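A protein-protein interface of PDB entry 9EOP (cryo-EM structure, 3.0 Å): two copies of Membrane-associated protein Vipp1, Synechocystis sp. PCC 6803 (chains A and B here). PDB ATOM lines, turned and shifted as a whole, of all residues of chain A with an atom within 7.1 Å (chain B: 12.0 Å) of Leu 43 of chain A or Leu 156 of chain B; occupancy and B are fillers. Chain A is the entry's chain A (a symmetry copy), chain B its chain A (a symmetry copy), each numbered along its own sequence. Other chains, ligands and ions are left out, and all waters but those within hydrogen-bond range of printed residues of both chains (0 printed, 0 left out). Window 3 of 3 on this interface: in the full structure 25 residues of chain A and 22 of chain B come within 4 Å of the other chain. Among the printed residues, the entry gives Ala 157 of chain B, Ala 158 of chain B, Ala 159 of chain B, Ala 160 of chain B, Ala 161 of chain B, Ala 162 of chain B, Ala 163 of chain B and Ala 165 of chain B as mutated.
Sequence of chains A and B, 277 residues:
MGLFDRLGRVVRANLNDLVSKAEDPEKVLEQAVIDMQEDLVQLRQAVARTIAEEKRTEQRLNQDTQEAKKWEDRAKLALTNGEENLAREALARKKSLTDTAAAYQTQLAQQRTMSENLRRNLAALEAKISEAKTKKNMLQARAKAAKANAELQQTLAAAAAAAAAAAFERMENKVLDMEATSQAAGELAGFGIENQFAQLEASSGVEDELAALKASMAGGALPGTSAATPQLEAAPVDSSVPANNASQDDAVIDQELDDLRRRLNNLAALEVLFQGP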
ATOM      1  N   GLU A  38      -1.427 -19.222  10.455  1.00  0.00           N
ATOM      2  CA  GLU A  38      -1.860 -18.488   9.272  1.00  0.00           C
ATOM      3  C   GLU A  38      -2.773 -17.314   9.596  1.00  0.00           C
ATOM      4  O   GLU A  38      -2.878 -16.385   8.791  1.00  0.00           O
ATOM      5  CB  GLU A  38      -2.573 -19.435   8.320  1.00  0.00           C
ATOM      6  CG  GLU A  38      -3.866 -19.953   8.868  1.00  0.00           C
ATOM      7  CD  GLU A  38      -4.510 -20.976   7.962  1.00  0.00           C
ATOM      8  OE1 GLU A  38      -3.773 -21.652   7.213  1.00  0.00           O
ATOM      9  OE2 GLU A  38      -5.751 -21.112   8.002  1.00  0.00           O
ATOM     10  N   ASP A  39      -3.437 -17.344  10.745  1.00  0.00           N
ATOM     11  CA  ASP A  39      -4.144 -16.171  11.248  1.00  0.00           C
ATOM     12  C   ASP A  39      -3.217 -14.984  11.460  1.00  0.00           C
ATOM     13  O   ASP A  39      -3.605 -13.834  11.229  1.00  0.00           O
ATOM     14  CB  ASP A  39      -4.839 -16.523  12.553  1.00  0.00           C
ATOM     15  CG  ASP A  39      -5.779 -15.444  13.019  1.00  0.00           C
ATOM     16  OD1 ASP A  39      -6.354 -14.740  12.162  1.00  0.00           O
ATOM     17  OD2 ASP A  39      -5.929 -15.287  14.248  1.00  0.00           O
ATOM     18  N   LEU A  40      -1.992 -15.240  11.899  1.00  0.00           N
ATOM     19  CA  LEU A  40      -1.004 -14.181  12.045  1.00  0.00           C
ATOM     20  C   LEU A  40      -0.528 -13.625  10.713  1.00  0.00           C
ATOM     21  O   LEU A  40      -0.206 -12.436  10.621  1.00  0.00           O
ATOM     22  CB  LEU A  40       0.176 -14.720  12.837  1.00  0.00           C
ATOM     23  CG  LEU A  40       1.423 -13.863  12.914  1.00  0.00           C
ATOM     24  CD1 LEU A  40       1.125 -12.591  13.620  1.00  0.00           C
ATOM     25  CD2 LEU A  40       2.494 -14.607  13.636  1.00  0.00           C
ATOM     26  N   VAL A  41      -0.454 -14.454   9.680  1.00  0.00           N
ATOM     27  CA  VAL A  41      -0.086 -13.964   8.356  1.00  0.00           C
ATOM     28  C   VAL A  41      -1.126 -12.984   7.826  1.00  0.00           C
ATOM     29  O   VAL A  41      -0.791 -11.910   7.316  1.00  0.00           O
ATOM     30  CB  VAL A  41       0.102 -15.149   7.397  1.00  0.00           C
ATOM     31  CG1 VAL A  41       0.394 -14.672   6.013  1.00  0.00           C
ATOM     32  CG2 VAL A  41       1.209 -16.017   7.882  1.00  0.00           C
ATOM     33  N   GLN A  42      -2.401 -13.343   7.937  1.00  0.00           N
ATOM     34  CA  GLN A  42      -3.474 -12.454   7.505  1.00  0.00           C
ATOM     35  C   GLN A  42      -3.503 -11.160   8.303  1.00  0.00           C
ATOM     36  O   GLN A  42      -3.684 -10.076   7.740  1.00  0.00           O
ATOM     37  CB  GLN A  42      -4.808 -13.174   7.624  1.00  0.00           C
ATOM     38  CG  GLN A  42      -4.920 -14.396   6.758  1.00  0.00           C
ATOM     39  CD  GLN A  42      -4.756 -14.088   5.291  1.00  0.00           C
ATOM     40  OE1 GLN A  42      -5.109 -13.006   4.828  1.00  0.00           O
ATOM     41  NE2 GLN A  42      -4.210 -15.040   4.547  1.00  0.00           N
ATOM     42  N   LEU A  43      -3.329 -11.255   9.616  1.00  0.00           N
ATOM     43  CA  LEU A  43      -3.312 -10.072  10.465  1.00  0.00           C
ATOM     44  C   LEU A  43      -2.184  -9.123  10.091  1.00  0.00           C
ATOM     45  O   LEU A  43      -2.379  -7.904  10.011  1.00  0.00           O
ATOM     46  CB  LEU A  43      -3.166 -10.505  11.917  1.00  0.00           C
ATOM     47  CG  LEU A  43      -3.111  -9.395  12.952  1.00  0.00           C
ATOM     48  CD1 LEU A  43      -4.423  -8.674  12.984  1.00  0.00           C
ATOM     49  CD2 LEU A  43      -2.777  -9.941  14.302  1.00  0.00           C
ATOM     50  N   ARG A  44      -0.997  -9.665   9.866  1.00  0.00           N
ATOM     51  CA  ARG A  44       0.168  -8.849   9.555  1.00  0.00           C
ATOM     52  C   ARG A  44      -0.027  -8.025   8.288  1.00  0.00           C
ATOM     53  O   ARG A  44       0.388  -6.862   8.226  1.00  0.00           O
ATOM     54  CB  ARG A  44       1.381  -9.759   9.436  1.00  0.00           C
ATOM     55  CG  ARG A  44       2.677  -9.039   9.303  1.00  0.00           C
ATOM     56  CD  ARG A  44       3.841  -9.987   9.186  1.00  0.00           C
ATOM     57  NE  ARG A  44       4.148 -10.626  10.458  1.00  0.00           N
ATOM     58  CZ  ARG A  44       4.362 -11.923  10.630  1.00  0.00           C
ATOM     59  NH1 ARG A  44       4.159 -12.796   9.658  1.00  0.00           N
ATOM     60  NH2 ARG A  44       4.775 -12.355  11.814  1.00  0.00           N
ATOM     61  N   GLN A  45      -0.655  -8.604   7.270  1.00  0.00           N
ATOM     62  CA  GLN A  45      -0.981  -7.862   6.057  1.00  0.00           C
ATOM     63  C   GLN A  45      -1.931  -6.703   6.328  1.00  0.00           C
ATOM     64  O   GLN A  45      -1.713  -5.582   5.859  1.00  0.00           O
ATOM     65  CB  GLN A  45      -1.620  -8.805   5.051  1.00  0.00           C
ATOM     66  CG  GLN A  45      -0.722  -9.891   4.557  1.00  0.00           C
ATOM     67  CD  GLN A  45      -1.426 -10.804   3.582  1.00  0.00           C
ATOM     68  OE1 GLN A  45      -2.551 -10.532   3.165  1.00  0.00           O
ATOM     69  NE2 GLN A  45      -0.775 -11.900   3.223  1.00  0.00           N
ATOM     70  N   ALA A  46      -2.996  -6.962   7.076  1.00  0.00           N
ATOM     71  CA  ALA A  46      -3.976  -5.930   7.391  1.00  0.00           C
ATOM     72  C   ALA A  46      -3.380  -4.779   8.189  1.00  0.00           C
ATOM     73  O   ALA A  46      -3.701  -3.613   7.938  1.00  0.00           O
ATOM     74  CB  ALA A  46      -5.134  -6.552   8.150  1.00  0.00           C
ATOM     75  N   VAL A  47      -2.520  -5.076   9.157  1.00  0.00           N
ATOM     76  CA  VAL A  47      -1.836  -4.019   9.891  1.00  0.00           C
ATOM     77  C   VAL A  47      -0.977  -3.179   8.958  1.00  0.00           C
ATOM     78  O   VAL A  47      -1.045  -1.945   8.967  1.00  0.00           O
ATOM     79  CB  VAL A  47      -0.989  -4.625  11.019  1.00  0.00           C
ATOM     80  CG1 VAL A  47      -0.134  -3.579  11.657  1.00  0.00           C
ATOM     81  CG2 VAL A  47      -1.861  -5.276  12.020  1.00  0.00           C
ATOM     82  N   ALA A  48      -0.155  -3.830   8.144  1.00  0.00           N
ATOM     83  CA  ALA A  48       0.754  -3.098   7.275  1.00  0.00           C
ATOM     84  C   ALA A  48       0.010  -2.171   6.335  1.00  0.00           C
ATOM     85  O   ALA A  48       0.516  -1.101   5.981  1.00  0.00           O
ATOM     86  CB  ALA A  48       1.585  -4.083   6.471  1.00  0.00           C
ATOM     87  N   ARG A  49      -1.185  -2.563   5.925  1.00  0.00           N
ATOM     88  CA  ARG A  49      -2.044  -1.747   5.088  1.00  0.00           C
ATOM     89  C   ARG A  49      -2.586  -0.513   5.794  1.00  0.00           C
ATOM     90  O   ARG A  49      -3.147   0.357   5.122  1.00  0.00           O
ATOM     91  CB  ARG A  49      -3.159  -2.632   4.559  1.00  0.00           C
ATOM     92  CG  ARG A  49      -4.141  -1.962   3.671  1.00  0.00           C
ATOM     93  CD  ARG A  49      -4.627  -2.905   2.586  1.00  0.00           C
ATOM     94  NE  ARG A  49      -4.839  -4.272   3.040  1.00  0.00           N
ATOM     95  CZ  ARG A  49      -5.854  -4.675   3.793  1.00  0.00           C
ATOM     96  NH1 ARG A  49      -6.740  -3.820   4.272  1.00  0.00           N
ATOM     97  NH2 ARG A  49      -5.978  -5.969   4.074  1.00  0.00           N
ATOM     98  N   LEU A 118      -1.726  -2.019  17.924  1.00  0.00           N
ATOM     99  CA  LEU A 118      -1.710  -3.208  17.079  1.00  0.00           C
ATOM    100  C   LEU A 118      -0.353  -3.885  17.059  1.00  0.00           C
ATOM    101  O   LEU A 118      -0.260  -5.118  17.066  1.00  0.00           O
ATOM    102  CB  LEU A 118      -2.098  -2.814  15.665  1.00  0.00           C
ATOM    103  CG  LEU A 118      -3.549  -2.425  15.456  1.00  0.00           C
ATOM    104  CD1 LEU A 118      -3.724  -1.882  14.074  1.00  0.00           C
ATOM    105  CD2 LEU A 118      -4.445  -3.606  15.676  1.00  0.00           C
ATOM    106  N   ASN A 121       0.058  -5.954  20.169  1.00  0.00           N
ATOM    107  CA  ASN A 121      -0.792  -7.137  20.083  1.00  0.00           C
ATOM    108  C   ASN A 121      -0.221  -8.188  19.143  1.00  0.00           C
ATOM    109  O   ASN A 121      -0.335  -9.391  19.396  1.00  0.00           O
ATOM    110  CB  ASN A 121      -2.190  -6.736  19.626  1.00  0.00           C
ATOM    111  CG  ASN A 121      -3.048  -6.245  20.762  1.00  0.00           C
ATOM    112  OD1 ASN A 121      -3.666  -7.033  21.477  1.00  0.00           O
ATOM    113  ND2 ASN A 121      -3.083  -4.935  20.949  1.00  0.00           N
ATOM    114  N   LEU A 122       0.383  -7.749  18.052  1.00  0.00           N
ATOM    115  CA  LEU A 122       0.960  -8.659  17.074  1.00  0.00           C
ATOM    116  C   LEU A 122       2.148  -9.435  17.629  1.00  0.00           C
ATOM    117  O   LEU A 122       2.326 -10.615  17.315  1.00  0.00           O
ATOM    118  CB  LEU A 122       1.358  -7.847  15.851  1.00  0.00           C
ATOM    119  CG  LEU A 122       1.817  -8.518  14.578  1.00  0.00           C
ATOM    120  CD1 LEU A 122       0.743  -9.401  14.053  1.00  0.00           C
ATOM    121  CD2 LEU A 122       2.106  -7.435  13.592  1.00  0.00           C
ATOM    122  N   LEU A 125       0.962 -12.239  20.182  1.00  0.00           N
ATOM    123  CA  LEU A 125       0.408 -13.462  19.617  1.00  0.00           C
ATOM    124  C   LEU A 125       1.478 -14.508  19.329  1.00  0.00           C
ATOM    125  O   LEU A 125       1.401 -15.640  19.817  1.00  0.00           O
ATOM    126  CB  LEU A 125      -0.364 -13.121  18.350  1.00  0.00           C
ATOM    127  CG  LEU A 125      -0.848 -14.285  17.503  1.00  0.00           C
ATOM    128  CD1 LEU A 125      -1.716 -15.214  18.304  1.00  0.00           C
ATOM    129  CD2 LEU A 125      -1.610 -13.744  16.333  1.00  0.00           C
ATOM    130  N   LYS B 147     -11.791   2.405   5.207  1.00  0.00           N
ATOM    131  CA  LYS B 147     -11.972   1.097   4.599  1.00  0.00           C
ATOM    132  C   LYS B 147     -10.873   0.108   4.957  1.00  0.00           C
ATOM    133  O   LYS B 147     -11.121  -1.101   4.991  1.00  0.00           O
ATOM    134  CB  LYS B 147     -12.067   1.284   3.096  1.00  0.00           C
ATOM    135  CG  LYS B 147     -12.416   0.065   2.318  1.00  0.00           C
ATOM    136  CD  LYS B 147     -13.115   0.457   1.022  1.00  0.00           C
ATOM    137  CE  LYS B 147     -12.375   1.545   0.259  1.00  0.00           C
ATOM    138  NZ  LYS B 147     -13.143   1.995  -0.929  1.00  0.00           N
ATOM    139  N   ALA B 148      -9.665   0.592   5.209  1.00  0.00           N
ATOM    140  CA  ALA B 148      -8.606  -0.263   5.727  1.00  0.00           C
ATOM    141  C   ALA B 148      -8.896  -0.767   7.134  1.00  0.00           C
ATOM    142  O   ALA B 148      -8.659  -1.940   7.438  1.00  0.00           O
ATOM    143  CB  ALA B 148      -7.292   0.500   5.711  1.00  0.00           C
ATOM    144  N   ASN B 149      -9.405   0.099   8.005  1.00  0.00           N
ATOM    145  CA  ASN B 149      -9.781  -0.319   9.349  1.00  0.00           C
ATOM    146  C   ASN B 149     -10.961  -1.278   9.375  1.00  0.00           C
ATOM    147  O   ASN B 149     -11.030  -2.145  10.250  1.00  0.00           O
ATOM    148  CB  ASN B 149     -10.113   0.912  10.171  1.00  0.00           C
ATOM    149  CG  ASN B 149      -8.911   1.750  10.463  1.00  0.00           C
ATOM    150  OD1 ASN B 149      -8.678   2.777   9.829  1.00  0.00           O
ATOM    151  ND2 ASN B 149      -8.138   1.330  11.446  1.00  0.00           N
ATOM    152  N   ALA B 150     -11.894  -1.143   8.441  1.00  0.00           N
ATOM    153  CA  ALA B 150     -12.992  -2.094   8.345  1.00  0.00           C
ATOM    154  C   ALA B 150     -12.516  -3.513   8.067  1.00  0.00           C
ATOM    155  O   ALA B 150     -13.014  -4.471   8.666  1.00  0.00           O
ATOM    156  CB  ALA B 150     -13.954  -1.644   7.257  1.00  0.00           C
ATOM    157  N   GLU B 151     -11.557  -3.668   7.162  1.00  0.00           N
ATOM    158  CA  GLU B 151     -11.006  -4.984   6.857  1.00  0.00           C
ATOM    159  C   GLU B 151     -10.214  -5.569   8.017  1.00  0.00           C
ATOM    160  O   GLU B 151     -10.224  -6.784   8.230  1.00  0.00           O
ATOM    161  CB  GLU B 151     -10.128  -4.884   5.621  1.00  0.00           C
ATOM    162  CG  GLU B 151     -10.898  -4.582   4.364  1.00  0.00           C
ATOM    163  CD  GLU B 151      -9.999  -4.386   3.164  1.00  0.00           C
ATOM    164  OE1 GLU B 151      -8.783  -4.640   3.283  1.00  0.00           O
ATOM    165  OE2 GLU B 151     -10.508  -3.970   2.101  1.00  0.00           O
ATOM    166  N   LEU B 152      -9.514  -4.726   8.766  1.00  0.00           N
ATOM    167  CA  LEU B 152      -8.816  -5.192   9.955  1.00  0.00           C
ATOM    168  C   LEU B 152      -9.773  -5.702  11.021  1.00  0.00           C
ATOM    169  O   LEU B 152      -9.589  -6.797  11.562  1.00  0.00           O
ATOM    170  CB  LEU B 152      -7.975  -4.058  10.517  1.00  0.00           C
ATOM    171  CG  LEU B 152      -7.103  -4.361  11.722  1.00  0.00           C
ATOM    172  CD1 LEU B 152      -5.944  -3.450  11.708  1.00  0.00           C
ATOM    173  CD2 LEU B 152      -7.851  -4.182  13.003  1.00  0.00           C
ATOM    174  N   GLN B 153     -10.801  -4.924  11.336  1.00  0.00           N
ATOM    175  CA  GLN B 153     -11.745  -5.324  12.369  1.00  0.00           C
ATOM    176  C   GLN B 153     -12.514  -6.578  11.991  1.00  0.00           C
ATOM    177  O   GLN B 153     -12.842  -7.392  12.860  1.00  0.00           O
ATOM    178  CB  GLN B 153     -12.707  -4.175  12.634  1.00  0.00           C
ATOM    179  CG  GLN B 153     -12.049  -2.952  13.232  1.00  0.00           C
ATOM    180  CD  GLN B 153     -11.396  -3.224  14.564  1.00  0.00           C
ATOM    181  OE1 GLN B 153     -11.723  -4.195  15.245  1.00  0.00           O
ATOM    182  NE2 GLN B 153     -10.449  -2.375  14.937  1.00  0.00           N
ATOM    183  N   GLN B 154     -12.807  -6.752  10.708  1.00  0.00           N
ATOM    184  CA  GLN B 154     -13.401  -7.993  10.229  1.00  0.00           C
ATOM    185  C   GLN B 154     -12.476  -9.186  10.421  1.00  0.00           C
ATOM    186  O   GLN B 154     -12.924 -10.278  10.785  1.00  0.00           O
ATOM    187  CB  GLN B 154     -13.768  -7.837   8.761  1.00  0.00           C
ATOM    188  CG  GLN B 154     -14.415  -9.043   8.156  1.00  0.00           C
ATOM    189  CD  GLN B 154     -14.825  -8.807   6.722  1.00  0.00           C
ATOM    190  OE1 GLN B 154     -14.528  -7.761   6.145  1.00  0.00           O
ATOM    191  NE2 GLN B 154     -15.506  -9.780   6.133  1.00  0.00           N
ATOM    192  N   THR B 155     -11.185  -9.000  10.170  1.00  0.00           N
ATOM    193  CA  THR B 155     -10.214 -10.072  10.354  1.00  0.00           C
ATOM    194  C   THR B 155     -10.072 -10.476  11.816  1.00  0.00           C
ATOM    195  O   THR B 155     -10.009 -11.670  12.134  1.00  0.00           O
ATOM    196  CB  THR B 155      -8.868  -9.619   9.794  1.00  0.00           C
ATOM    197  OG1 THR B 155      -9.013  -9.303   8.406  1.00  0.00           O
ATOM    198  CG2 THR B 155      -7.829 -10.677   9.945  1.00  0.00           C
ATOM    199  N   LEU B 156     -10.013  -9.501  12.714  1.00  0.00           N
ATOM    200  CA  LEU B 156      -9.896  -9.780  14.141  1.00  0.00           C
ATOM    201  C   LEU B 156     -11.103 -10.528  14.691  1.00  0.00           C
ATOM    202  O   LEU B 156     -10.959 -11.398  15.557  1.00  0.00           O
ATOM    203  CB  LEU B 156      -9.711  -8.472  14.893  1.00  0.00           C
ATOM    204  CG  LEU B 156      -8.272  -8.123  15.213  1.00  0.00           C
ATOM    205  CD1 LEU B 156      -7.541  -8.021  13.939  1.00  0.00           C
ATOM    206  CD2 LEU B 156      -8.184  -6.821  15.924  1.00  0.00           C
ATOM    207  N   ALA B 157     -12.296 -10.200  14.212  1.00  0.00           N
ATOM    208  CA  ALA B 157     -13.496 -10.914  14.628  1.00  0.00           C
ATOM    209  C   ALA B 157     -13.521 -12.359  14.144  1.00  0.00           C
ATOM    210  O   ALA B 157     -13.847 -13.271  14.910  1.00  0.00           O
ATOM    211  CB  ALA B 157     -14.721 -10.173  14.112  1.00  0.00           C
ATOM    212  N   ALA B 158     -13.174 -12.590  12.883  1.00  0.00           N
ATOM    213  CA  ALA B 158     -13.143 -13.954  12.365  1.00  0.00           C
ATOM    214  C   ALA B 158     -12.150 -14.830  13.113  1.00  0.00           C
ATOM    215  O   ALA B 158     -12.420 -16.009  13.370  1.00  0.00           O
ATOM    216  CB  ALA B 158     -12.810 -13.932  10.879  1.00  0.00           C
ATOM    217  N   ALA B 159     -10.995 -14.279  13.471  1.00  0.00           N
ATOM    218  CA  ALA B 159     -10.018 -15.035  14.244  1.00  0.00           C
ATOM    219  C   ALA B 159     -10.530 -15.387  15.631  1.00  0.00           C
ATOM    220  O   ALA B 159     -10.290 -16.495  16.124  1.00  0.00           O
ATOM    221  CB  ALA B 159      -8.730 -14.233  14.359  1.00  0.00           C
ATOM    222  N   ALA B 160     -11.233 -14.463  16.278  1.00  0.00           N
ATOM    223  CA  ALA B 160     -11.810 -14.750  17.583  1.00  0.00           C
ATOM    224  C   ALA B 160     -12.954 -15.749  17.507  1.00  0.00           C
ATOM    225  O   ALA B 160     -13.231 -16.443  18.490  1.00  0.00           O
ATOM    226  CB  ALA B 160     -12.293 -13.456  18.224  1.00  0.00           C
ATOM    227  N   ALA B 161     -13.632 -15.833  16.366  1.00  0.00           N
ATOM    228  CA  ALA B 161     -14.693 -16.822  16.222  1.00  0.00           C
ATOM    229  C   ALA B 161     -14.162 -18.242  16.075  1.00  0.00           C
ATOM    230  O   ALA B 161     -14.871 -19.197  16.408  1.00  0.00           O
ATOM    231  CB  ALA B 161     -15.561 -16.475  15.021  1.00  0.00           C
ATOM    232  N   ALA B 162     -12.939 -18.413  15.574  1.00  0.00           N
ATOM    233  CA  ALA B 162     -12.389 -19.758  15.458  1.00  0.00           C
ATOM    234  C   ALA B 162     -11.905 -20.315  16.791  1.00  0.00           C
ATOM    235  O   ALA B 162     -12.037 -21.518  17.036  1.00  0.00           O
ATOM    236  CB  ALA B 162     -11.247 -19.759  14.449  1.00  0.00           C
ATOM    237  N   ALA B 163     -11.360 -19.469  17.657  1.00  0.00           N
ATOM    238  CA  ALA B 163     -10.970 -19.859  19.008  1.00  0.00           C
ATOM    239  C   ALA B 163     -10.102 -21.115  19.001  1.00  0.00           C
ATOM    240  O   ALA B 163     -10.358 -22.087  19.713  1.00  0.00           O
ATOM    241  CB  ALA B 163     -12.203 -20.058  19.876  1.00  0.00           C
ATOM    242  N   ALA B 164      -9.068 -21.088  18.166  1.00  0.00           N
ATOM    243  CA  ALA B 164      -8.092 -22.168  18.131  1.00  0.00           C
ATOM    244  C   ALA B 164      -7.417 -22.386  19.479  1.00  0.00           C
ATOM    245  O   ALA B 164      -7.070 -23.519  19.829  1.00  0.00           O
ATOM    246  CB  ALA B 164      -7.052 -21.868  17.065  1.00  0.00           C
ATOM    247  N   ALA B 165      -7.225 -21.316  20.245  1.00  0.00           N
ATOM    248  CA  ALA B 165      -6.657 -21.411  21.585  1.00  0.00           C
ATOM    249  C   ALA B 165      -7.547 -22.164  22.561  1.00  0.00           C
ATOM    250  O   ALA B 165      -7.037 -22.821  23.475  1.00  0.00           O
ATOM    251  CB  ALA B 165      -6.374 -20.016  22.119  1.00  0.00           C
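The side-chain carboxylate (OE1) of Glu 151 of chain B is in salt-bridge range of the guanidinium group (NH1) of Arg 49 of chain A (2.4 Å).
The backbone carbonyl oxygen of Glu 151 of chain B sits at hydrogen-bond distance from the side-chain hydroxyl of Thr 155 of chain B, at 2.8 Å.
Among the printed residues, merely in contact across the chains: Asp 39 of chain A with Ala 159 of chain B (3.0 Å), Leu 43 of chain A with Leu 156 of chain B (3.3 Å) and Leu 118 of chain A with Leu 152 of chain B (3.6 Å).
Of chain B, only Ala 159 (3.0 Å) comes within 4 Å of Asp 39 of chain A.
No residue of chain B comes within 4 Å of Leu 40 of chain A.
No residue of chain B comes within 4 Å of Val 41 of chain A.
Of chain B, only Leu 156 (3.3 Å) comes within 4 Å of Leu 43 of chain A.
Gln 45 of chain A touches none of the printed residues of chain B.
No residue of chain B comes within 4 Å of Ala 46 of chain A.
No residue of chain B comes within 4 Å of Val 47 of chain A.
Of the printed residues of chain B, Arg 49 of chain A touches Glu 151 (2.4 Å).
No residue of chain B comes within 4 Å of Leu 122 of chain A.
Printed residues of chain A within 4 Å of Glu 151 of chain B: Arg 49 (2.4 Å).
Leu 156 of chain B touches just one residue of chain A: Leu 43.
The nearest residue of chain B that does not touch Leu 43 of chain A is Thr 155 of chain B (4.5 Å).
The nearest residue of chain A that does not touch Leu 156 of chain B is Leu 118 of chain A (4.9 Å).
Of the 16 printed residues of chain A, 4 touch a printed residue of chain B.
Among the printed residues, 4 pairs touch across the chains.
No position is printed for both chains.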
